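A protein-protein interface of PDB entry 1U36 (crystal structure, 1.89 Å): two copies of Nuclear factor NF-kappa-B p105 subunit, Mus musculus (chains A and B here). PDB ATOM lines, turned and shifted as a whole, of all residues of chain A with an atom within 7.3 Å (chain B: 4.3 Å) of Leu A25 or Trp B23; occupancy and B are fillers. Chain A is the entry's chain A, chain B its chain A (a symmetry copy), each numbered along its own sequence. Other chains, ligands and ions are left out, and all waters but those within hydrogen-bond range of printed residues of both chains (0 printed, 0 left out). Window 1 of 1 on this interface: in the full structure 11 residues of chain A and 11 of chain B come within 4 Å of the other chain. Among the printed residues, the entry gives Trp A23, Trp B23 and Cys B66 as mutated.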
ATOM      1  N   LYS A   5       1.347   7.164  -0.601  1.00  0.00           N
ATOM      2  CA  LYS A   5       1.556   8.193  -1.591  1.00  0.00           C
ATOM      3  C   LYS A   5       2.283   7.662  -2.801  1.00  0.00           C
ATOM      4  O   LYS A   5       3.330   7.036  -2.663  1.00  0.00           O
ATOM      5  CB  LYS A   5       2.340   9.350  -1.002  1.00  0.00           C
ATOM      6  CG  LYS A   5       2.497  10.506  -1.962  1.00  0.00           C
ATOM      7  CD  LYS A   5       3.328  11.644  -1.358  1.00  0.00           C
ATOM      8  CE  LYS A   5       2.568  12.407  -0.267  1.00  0.00           C
ATOM      9  NZ  LYS A   5       3.361  13.521   0.346  1.00  0.00           N
ATOM     10  N   ILE A   6       1.677   7.884  -3.968  1.00  0.00           N
ATOM     11  CA  ILE A   6       2.335   7.747  -5.238  1.00  0.00           C
ATOM     12  C   ILE A   6       3.143   9.009  -5.499  1.00  0.00           C
ATOM     13  O   ILE A   6       2.605  10.073  -5.742  1.00  0.00           O
ATOM     14  CB  ILE A   6       1.338   7.479  -6.395  1.00  0.00           C
ATOM     15  CG1 ILE A   6       0.506   6.259  -6.071  1.00  0.00           C
ATOM     16  CG2 ILE A   6       2.163   7.241  -7.672  1.00  0.00           C
ATOM     17  CD1 ILE A   6      -0.572   5.953  -7.048  1.00  0.00           C
ATOM     18  N   VAL A   7       4.465   8.877  -5.448  1.00  0.00           N
ATOM     19  CA  VAL A   7       5.329  10.034  -5.601  1.00  0.00           C
ATOM     20  C   VAL A   7       5.517  10.337  -7.083  1.00  0.00           C
ATOM     21  O   VAL A   7       5.413  11.491  -7.522  1.00  0.00           O
ATOM     22  CB  VAL A   7       6.653   9.766  -4.850  1.00  0.00           C
ATOM     23  CG1 VAL A   7       7.716  10.814  -5.212  1.00  0.00           C
ATOM     24  CG2 VAL A   7       6.390   9.735  -3.345  1.00  0.00           C
ATOM     25  N   ARG A   8       5.756   9.300  -7.878  1.00  0.00           N
ATOM     26  CA  ARG A   8       5.907   9.435  -9.312  1.00  0.00           C
ATOM     27  C   ARG A   8       5.622   8.097  -9.945  1.00  0.00           C
ATOM     28  O   ARG A   8       5.735   7.070  -9.313  1.00  0.00           O
ATOM     29  CB  ARG A   8       7.369   9.758  -9.691  1.00  0.00           C
ATOM     30  CG  ARG A   8       7.886  11.143  -9.357  1.00  0.00           C
ATOM     31  CD  ARG A   8       9.123  11.521 -10.176  1.00  0.00           C
ATOM     32  NE  ARG A   8       8.794  11.430 -11.598  1.00  0.00           N
ATOM     33  CZ  ARG A   8       9.584  11.774 -12.601  1.00  0.00           C
ATOM     34  NH1 ARG A   8      10.807  12.264 -12.387  1.00  0.00           N
ATOM     35  NH2 ARG A   8       9.132  11.617 -13.843  1.00  0.00           N
ATOM     36  N   MET A   9       5.287   8.139 -11.213  1.00  0.00           N
ATOM     37  CA  MET A   9       5.141   6.968 -12.074  1.00  0.00           C
ATOM     38  C   MET A   9       5.913   7.181 -13.372  1.00  0.00           C
ATOM     39  O   MET A   9       5.967   8.296 -13.887  1.00  0.00           O
ATOM     40  CB  MET A   9       3.652   6.752 -12.397  1.00  0.00           C
ATOM     41  CG  MET A   9       2.853   6.435 -11.165  1.00  0.00           C
ATOM     42  SD  MET A   9       1.075   6.186 -11.573  1.00  0.00           S
ATOM     43  CE  MET A   9       1.128   4.773 -12.581  1.00  0.00           C
ATOM     44  N   ASP A  10       6.558   6.141 -13.918  1.00  0.00           N
ATOM     45  CA  ASP A  10       7.388   6.343 -15.124  1.00  0.00           C
ATOM     46  C   ASP A  10       6.559   6.321 -16.411  1.00  0.00           C
ATOM     47  O   ASP A  10       7.053   6.604 -17.487  1.00  0.00           O
ATOM     48  CB  ASP A  10       8.627   5.382 -15.174  1.00  0.00           C
ATOM     49  CG  ASP A  10       8.287   3.964 -15.457  1.00  0.00           C
ATOM     50  OD1 ASP A  10       7.092   3.585 -15.471  1.00  0.00           O
ATOM     51  OD2 ASP A  10       9.197   3.114 -15.717  1.00  0.00           O
ATOM     52  N   ARG A  11       5.284   6.003 -16.301  1.00  0.00           N
ATOM     53  CA  ARG A  11       4.346   5.987 -17.414  1.00  0.00           C
ATOM     54  C   ARG A  11       2.989   6.311 -16.806  1.00  0.00           C
ATOM     55  O   ARG A  11       2.660   5.758 -15.756  1.00  0.00           O
ATOM     56  CB  ARG A  11       4.238   4.583 -18.024  1.00  0.00           C
ATOM     57  CG  ARG A  11       5.180   4.260 -19.134  1.00  0.00           C
ATOM     58  CD  ARG A  11       4.822   4.962 -20.443  1.00  0.00           C
ATOM     59  NE  ARG A  11       3.812   4.277 -21.268  1.00  0.00           N
ATOM     60  CZ  ARG A  11       3.103   4.893 -22.232  1.00  0.00           C
ATOM     61  NH1 ARG A  11       2.224   4.210 -22.951  1.00  0.00           N
ATOM     62  NH2 ARG A  11       3.289   6.193 -22.487  1.00  0.00           N
ATOM     63  N   ILE A  22       4.965  -0.823 -15.606  1.00  0.00           N
ATOM     64  CA  ILE A  22       5.131   0.526 -15.127  1.00  0.00           C
ATOM     65  C   ILE A  22       5.800   0.444 -13.780  1.00  0.00           C
ATOM     66  O   ILE A  22       5.606  -0.527 -13.005  1.00  0.00           O
ATOM     67  CB  ILE A  22       3.718   1.249 -15.045  1.00  0.00           C
ATOM     68  CG1 ILE A  22       3.063   1.230 -16.434  1.00  0.00           C
ATOM     69  CG2 ILE A  22       3.833   2.678 -14.436  1.00  0.00           C
ATOM     70  CD1 ILE A  22       1.813   2.074 -16.607  1.00  0.00           C
ATOM     71  N   TRP A  23       6.585   1.465 -13.491  1.00  0.00           N
ATOM     72  CA  TRP A  23       7.201   1.633 -12.200  1.00  0.00           C
ATOM     73  C   TRP A  23       6.572   2.801 -11.498  1.00  0.00           C
ATOM     74  O   TRP A  23       6.307   3.832 -12.120  1.00  0.00           O
ATOM     75  CB  TRP A  23       8.685   1.915 -12.308  1.00  0.00           C
ATOM     76  CG  TRP A  23       9.486   0.765 -12.864  1.00  0.00           C
ATOM     77  CD1 TRP A  23       9.037  -0.367 -13.500  1.00  0.00           C
ATOM     78  CD2 TRP A  23      10.902   0.680 -12.842  1.00  0.00           C
ATOM     79  NE1 TRP A  23      10.106  -1.139 -13.888  1.00  0.00           N
ATOM     80  CE2 TRP A  23      11.264  -0.530 -13.464  1.00  0.00           C
ATOM     81  CE3 TRP A  23      11.904   1.480 -12.311  1.00  0.00           C
ATOM     82  CZ2 TRP A  23      12.606  -0.920 -13.599  1.00  0.00           C
ATOM     83  CZ3 TRP A  23      13.233   1.106 -12.466  1.00  0.00           C
ATOM     84  CH2 TRP A  23      13.567  -0.070 -13.076  1.00  0.00           C
ATOM     85  N   LEU A  24       6.395   2.656 -10.193  1.00  0.00           N
ATOM     86  CA  LEU A  24       6.039   3.785  -9.377  1.00  0.00           C
ATOM     87  C   LEU A  24       6.946   3.907  -8.153  1.00  0.00           C
ATOM     88  O   LEU A  24       7.461   2.930  -7.617  1.00  0.00           O
ATOM     89  CB  LEU A  24       4.536   3.758  -9.030  1.00  0.00           C
ATOM     90  CG  LEU A  24       3.933   2.785  -8.047  1.00  0.00           C
ATOM     91  CD1 LEU A  24       4.327   3.187  -6.618  1.00  0.00           C
ATOM     92  CD2 LEU A  24       2.407   2.766  -8.196  1.00  0.00           C
ATOM     93  N   LEU A  25       7.205   5.143  -7.776  1.00  0.00           N
ATOM     94  CA  LEU A  25       7.901   5.463  -6.551  1.00  0.00           C
ATOM     95  C   LEU A  25       6.824   5.815  -5.535  1.00  0.00           C
ATOM     96  O   LEU A  25       5.864   6.541  -5.857  1.00  0.00           O
ATOM     97  CB  LEU A  25       8.804   6.667  -6.801  1.00  0.00           C
ATOM     98  CG  LEU A  25       9.783   6.546  -7.977  1.00  0.00           C
ATOM     99  CD1 LEU A  25      10.663   7.770  -8.130  1.00  0.00           C
ATOM    100  CD2 LEU A  25      10.594   5.255  -7.889  1.00  0.00           C
ATOM    101  N   CYS A  26       7.002   5.347  -4.309  1.00  0.00           N
ATOM    102  CA  CYS A  26       6.034   5.576  -3.264  1.00  0.00           C
ATOM    103  C   CYS A  26       6.704   5.950  -1.970  1.00  0.00           C
ATOM    104  O   CYS A  26       7.907   5.701  -1.795  1.00  0.00           O
ATOM    105  CB  CYS A  26       5.203   4.309  -3.077  1.00  0.00           C
ATOM    106  SG  CYS A  26       6.087   2.747  -2.908  1.00  0.00           S
ATOM    107  N   ASP A  27       5.919   6.494  -1.036  1.00  0.00           N
ATOM    108  CA  ASP A  27       6.331   6.526   0.373  1.00  0.00           C
ATOM    109  C   ASP A  27       6.357   5.084   0.833  1.00  0.00           C
ATOM    110  O   ASP A  27       5.911   4.188   0.121  1.00  0.00           O
ATOM    111  CB  ASP A  27       5.348   7.349   1.246  1.00  0.00           C
ATOM    112  CG  ASP A  27       5.463   8.855   1.048  1.00  0.00           C
ATOM    113  OD1 ASP A  27       6.409   9.357   0.381  1.00  0.00           O
ATOM    114  OD2 ASP A  27       4.630   9.641   1.554  1.00  0.00           O
ATOM    115  N   PHE A  63       9.984   1.146  -1.263  1.00  0.00           N
ATOM    116  CA  PHE A  63       9.899   2.515  -1.775  1.00  0.00           C
ATOM    117  C   PHE A  63       9.612   2.627  -3.291  1.00  0.00           C
ATOM    118  O   PHE A  63       9.518   3.730  -3.851  1.00  0.00           O
ATOM    119  CB  PHE A  63      11.199   3.242  -1.431  1.00  0.00           C
ATOM    120  CG  PHE A  63      11.265   3.705   0.006  1.00  0.00           C
ATOM    121  CD1 PHE A  63      10.367   4.651   0.469  1.00  0.00           C
ATOM    122  CD2 PHE A  63      12.217   3.195   0.878  1.00  0.00           C
ATOM    123  CE1 PHE A  63      10.377   5.069   1.805  1.00  0.00           C
ATOM    124  CE2 PHE A  63      12.254   3.623   2.225  1.00  0.00           C
ATOM    125  CZ  PHE A  63      11.337   4.563   2.679  1.00  0.00           C
ATOM    126  N   ALA A  64       9.528   1.495  -3.959  1.00  0.00           N
ATOM    127  CA  ALA A  64       9.126   1.491  -5.359  1.00  0.00           C
ATOM    128  C   ALA A  64       8.485   0.185  -5.678  1.00  0.00           C
ATOM    129  O   ALA A  64       8.733  -0.818  -5.012  1.00  0.00           O
ATOM    130  CB  ALA A  64      10.305   1.746  -6.313  1.00  0.00           C
ATOM    131  N   ILE A  65       7.668   0.190  -6.718  1.00  0.00           N
ATOM    132  CA  ILE A  65       6.966  -1.010  -7.167  1.00  0.00           C
ATOM    133  C   ILE A  65       6.986  -1.108  -8.682  1.00  0.00           C
ATOM    134  O   ILE A  65       6.625  -0.158  -9.396  1.00  0.00           O
ATOM    135  CB  ILE A  65       5.494  -1.006  -6.670  1.00  0.00           C
ATOM    136  CG1 ILE A  65       5.414  -0.771  -5.153  1.00  0.00           C
ATOM    137  CG2 ILE A  65       4.819  -2.328  -7.044  1.00  0.00           C
ATOM    138  CD1 ILE A  65       3.919  -0.616  -4.682  1.00  0.00           C
ATOM    139  N   LEU A  87      -2.521   3.750  -4.593  1.00  0.00           N
ATOM    140  CA  LEU A  87      -2.110   2.692  -3.689  1.00  0.00           C
ATOM    141  C   LEU A  87      -3.243   2.390  -2.719  1.00  0.00           C
ATOM    142  O   LEU A  87      -3.987   3.282  -2.346  1.00  0.00           O
ATOM    143  CB  LEU A  87      -0.874   3.080  -2.880  1.00  0.00           C
ATOM    144  CG  LEU A  87       0.355   3.304  -3.750  1.00  0.00           C
ATOM    145  CD1 LEU A  87       1.412   4.118  -3.027  1.00  0.00           C
ATOM    146  CD2 LEU A  87       0.894   1.964  -4.225  1.00  0.00           C
ATOM    147  N   MET B   9      16.815  -1.274 -14.284  1.00  0.00           N
ATOM    148  CA  MET B   9      16.596  -0.029 -15.015  1.00  0.00           C
ATOM    149  C   MET B   9      15.335  -0.141 -15.865  1.00  0.00           C
ATOM    150  O   MET B   9      15.041  -1.207 -16.403  1.00  0.00           O
ATOM    151  CB  MET B   9      17.804   0.245 -15.930  1.00  0.00           C
ATOM    152  CG  MET B   9      19.063   0.467 -15.142  1.00  0.00           C
ATOM    153  SD  MET B   9      20.494   0.787 -16.255  1.00  0.00           S
ATOM    154  CE  MET B   9      20.039   2.283 -17.011  1.00  0.00           C
ATOM    155  N   ASP B  10      14.538   0.930 -15.983  1.00  0.00           N
ATOM    156  CA  ASP B  10      13.265   0.819 -16.724  1.00  0.00           C
ATOM    157  C   ASP B  10      13.455   0.973 -18.235  1.00  0.00           C
ATOM    158  O   ASP B  10      12.539   0.777 -19.011  1.00  0.00           O
ATOM    159  CB  ASP B  10      12.146   1.756 -16.147  1.00  0.00           C
ATOM    160  CG  ASP B  10      12.358   3.199 -16.421  1.00  0.00           C
ATOM    161  OD1 ASP B  10      13.438   3.603 -16.918  1.00  0.00           O
ATOM    162  OD2 ASP B  10      11.443   4.050 -16.186  1.00  0.00           O
ATOM    163  N   GLU B  21      14.635  10.469 -20.003  1.00  0.00           N
ATOM    164  CA  GLU B  21      14.506  10.082 -18.607  1.00  0.00           C
ATOM    165  C   GLU B  21      14.507   8.547 -18.445  1.00  0.00           C
ATOM    166  O   GLU B  21      13.724   7.839 -19.090  1.00  0.00           O
ATOM    167  CB  GLU B  21      13.250  10.684 -17.981  1.00  0.00           C
ATOM    168  CG  GLU B  21      13.059  10.294 -16.517  1.00  0.00           C
ATOM    169  CD  GLU B  21      12.106  11.204 -15.766  1.00  0.00           C
ATOM    170  OE1 GLU B  21      11.882  12.327 -16.221  1.00  0.00           O
ATOM    171  OE2 GLU B  21      11.601  10.792 -14.710  1.00  0.00           O
ATOM    172  N   ILE B  22      15.386   8.048 -17.567  1.00  0.00           N
ATOM    173  CA  ILE B  22      15.415   6.658 -17.185  1.00  0.00           C
ATOM    174  C   ILE B  22      15.397   6.606 -15.679  1.00  0.00           C
ATOM    175  O   ILE B  22      15.927   7.508 -14.982  1.00  0.00           O
ATOM    176  CB  ILE B  22      16.709   5.960 -17.787  1.00  0.00           C
ATOM    177  CG1 ILE B  22      16.701   6.116 -19.315  1.00  0.00           C
ATOM    178  CG2 ILE B  22      16.841   4.479 -17.318  1.00  0.00           C
ATOM    179  CD1 ILE B  22      17.734   5.315 -20.086  1.00  0.00           C
ATOM    180  N   TRP B  23      14.794   5.547 -15.171  1.00  0.00           N
ATOM    181  CA  TRP B  23      14.794   5.252 -13.762  1.00  0.00           C
ATOM    182  C   TRP B  23      15.640   4.040 -13.508  1.00  0.00           C
ATOM    183  O   TRP B  23      15.590   3.074 -14.272  1.00  0.00           O
ATOM    184  CB  TRP B  23      13.404   4.951 -13.242  1.00  0.00           C
ATOM    185  CG  TRP B  23      12.465   6.130 -13.291  1.00  0.00           C
ATOM    186  CD1 TRP B  23      12.618   7.323 -13.956  1.00  0.00           C
ATOM    187  CD2 TRP B  23      11.199   6.184 -12.652  1.00  0.00           C
ATOM    188  NE1 TRP B  23      11.501   8.105 -13.772  1.00  0.00           N
ATOM    189  CE2 TRP B  23      10.628   7.437 -12.945  1.00  0.00           C
ATOM    190  CE3 TRP B  23      10.510   5.320 -11.813  1.00  0.00           C
ATOM    191  CZ2 TRP B  23       9.368   7.810 -12.450  1.00  0.00           C
ATOM    192  CZ3 TRP B  23       9.252   5.679 -11.343  1.00  0.00           C
ATOM    193  CH2 TRP B  23       8.711   6.898 -11.641  1.00  0.00           C
ATOM    194  N   LEU B  24      16.367   4.071 -12.401  1.00  0.00           N
ATOM    195  CA  LEU B  24      17.018   2.882 -11.924  1.00  0.00           C
ATOM    196  C   LEU B  24      16.728   2.633 -10.444  1.00  0.00           C
ATOM    197  O   LEU B  24      16.516   3.548  -9.653  1.00  0.00           O
ATOM    198  CB  LEU B  24      18.525   2.908 -12.260  1.00  0.00           C
ATOM    199  CG  LEU B  24      19.513   3.802 -11.553  1.00  0.00           C
ATOM    200  CD1 LEU B  24      19.769   3.267 -10.136  1.00  0.00           C
ATOM    201  CD2 LEU B  24      20.824   3.865 -12.345  1.00  0.00           C
ATOM    202  N   HIS B  60      15.305   8.925  -4.935  1.00  0.00           N
ATOM    203  CA  HIS B  60      14.122   8.634  -4.133  1.00  0.00           C
ATOM    204  C   HIS B  60      14.443   7.743  -2.942  1.00  0.00           C
ATOM    205  O   HIS B  60      14.632   6.525  -3.078  1.00  0.00           O
ATOM    206  CB  HIS B  60      13.029   8.009  -5.009  1.00  0.00           C
ATOM    207  CG  HIS B  60      11.829   7.541  -4.244  1.00  0.00           C
ATOM    208  ND1 HIS B  60      10.911   8.419  -3.690  1.00  0.00           N
ATOM    209  CD2 HIS B  60      11.389   6.294  -3.951  1.00  0.00           C
ATOM    210  CE1 HIS B  60       9.976   7.719  -3.062  1.00  0.00           C
ATOM    211  NE2 HIS B  60      10.238   6.428  -3.214  1.00  0.00           N
ATOM    212  N   ALA B  64      16.265   4.609  -5.349  1.00  0.00           N
ATOM    213  CA  ALA B  64      16.022   4.746  -6.779  1.00  0.00           C
ATOM    214  C   ALA B  64      16.488   6.087  -7.226  1.00  0.00           C
ATOM    215  O   ALA B  64      16.573   7.022  -6.432  1.00  0.00           O
ATOM    216  CB  ALA B  64      14.541   4.553  -7.147  1.00  0.00           C
ATOM    217  N   ILE B  65      16.774   6.192  -8.513  1.00  0.00           N
ATOM    218  CA  ILE B  65      17.237   7.441  -9.113  1.00  0.00           C
ATOM    219  C   ILE B  65      16.566   7.674 -10.455  1.00  0.00           C
ATOM    220  O   ILE B  65      16.562   6.798 -11.336  1.00  0.00           O
ATOM    221  CB  ILE B  65      18.779   7.423  -9.304  1.00  0.00           C
ATOM    222  CG1 ILE B  65      19.502   7.055  -7.999  1.00  0.00           C
ATOM    223  CG2 ILE B  65      19.252   8.787  -9.814  1.00  0.00           C
ATOM    224  CD1 ILE B  65      21.050   6.890  -8.237  1.00  0.00           C
ATOM    225  N   CYS B  66      15.983   8.863 -10.624  1.00  0.00           N
ATOM    226  CA  CYS B  66      15.418   9.254 -11.905  1.00  0.00           C
ATOM    227  C   CYS B  66      16.411  10.225 -12.498  1.00  0.00           C
ATOM    228  O   CYS B  66      16.807  11.200 -11.840  1.00  0.00           O
ATOM    229  CB  CYS B  66      14.076   9.975 -11.731  1.00  0.00           C
ATOM    230  SG  CYS B  66      12.942   9.130 -10.619  1.00  0.00           S
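Of chain B, only Trp B23, His B60 and Cys B66 come within 4 Å of Leu A25.
Of chain A, only Arg A8 (3.7 Å), Met A9 (3.3 Å), Asp A10 (3.2 Å), Trp A23 (3.6 Å) and Leu A25 (3.5 Å) come within 4 Å of Trp B23.
Printed residues of chain B within 4 Å of Met A9: Trp B23.
Printed residues of chain B within 4 Å of Phe A63: His B60 (2.9 Å).
Of the printed residues of chain A, Glu B21 touches Arg A8 (2.7 Å).
Of the printed residues of chain B, Arg A8 touches Glu B21 (2.7 Å) and Trp B23 (3.7 Å).
Of the printed residues of chain B, Cys A26 touches His B60.
Ile A65 touches none of the printed residues of chain B.
The nearest residue of chain B that does not touch Leu A25 is Ala B64 (4.1 Å).
The nearest residue of chain A that does not touch Trp B23 is Leu A24 (4.2 Å).
Arg A8 touches Trp B23 (CB to CH2, 3.7 Å).
C of Met A9 touches CH2 of Trp B23, 3.3 Å away.
Trp B23 touches Asp A10 (CH2 to N, 3.2 Å).
Trp A23 touches Met B9 (CH2 to C, 3.3 Å).
CH2 of Trp A23 touches N of Asp B10, 3.2 Å away.
Trp B23 touches Trp A23 (CZ3 to O, 3.6 Å).
Trp B23 touches Leu A25 (CZ3 to CG, 3.5 Å).
Leu A25 touches His B60 (CB to CD2, 3.9 Å).
Cys B66 touches Leu A25.
The guanidinium group of Arg A8 lies within salt-bridge range of the side-chain carboxylate of Glu B21, 2.7 Å away.
The side-chain carboxylate (OD2) of Asp B10 lies close to the side-chain carboxylate (OD2) of Asp A10 (2.5 Å).
NE2 of His B60 sits at hydrogen-bond distance from O of Cys A26 (2.8 Å).
The backbone carbonyl oxygen of Phe A63 is in hydrogen-bond range of a ring nitrogen (NE2) of His B60 (2.9 Å).
Met A9 touches Trp B23, and with the chains exchanged Trp A23 touches Met B9.
Asp A10 touches its own counterpart, Asp B10.
Asp A10 touches Trp B23, and with the chains exchanged Trp A23 touches Asp B10.
Trp A23 touches its own counterpart, Trp B23.
Positions printed for both chains: 9, 10, 22, 23, 24, 64 and 65.
Of the 13 pairs that touch across the chains among the printed residues, 6 have their exchanged pair printed and touching as well.
Hydrophobic or aromatic side chains of chain B within 4 Å of the printed part of chain A: Trp B23 and His B60.
Of the 17 printed residues of chain A, 7 touch a printed residue of chain B.
Hydrophobic or aromatic side chains of chain A that line the printed part of chain B: Trp A23, Leu A25 and Phe A63.
Along chain A the printed residues that touch a printed residue of chain B span positions 8 to 63.
Among the printed residues, 13 pairs touch across the chains.
Among the printed residues, Asp or Glu carboxylates within 4 Å of a Lys or Arg side-chain nitrogen of the other chain: Arg A8 with Glu B21.
N of Val A7 is in hydrogen-bond range of O of Leu A25, at 2.8 Å.
The backbone NH (N) of Asp A10 sits at hydrogen-bond distance from the backbone carbonyl oxygen (O) of Trp A23 (2.9 Å).
N of Cys A26 lies within hydrogen-bond range of O of Phe A63, at 3.0 Å.
The backbone carbonyl oxygen (O) of Trp B23 lies within hydrogen-bond range of the backbone NH (N) of Asp B10.
The side-chain carboxylate (OE2) of Glu B21 sits at hydrogen-bond distance from the indole nitrogen (NE1) of Trp B23 (2.8 Å).
SG of Cys B66 is in hydrogen-bond range of NE1 of Trp B23 (3.6 Å).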
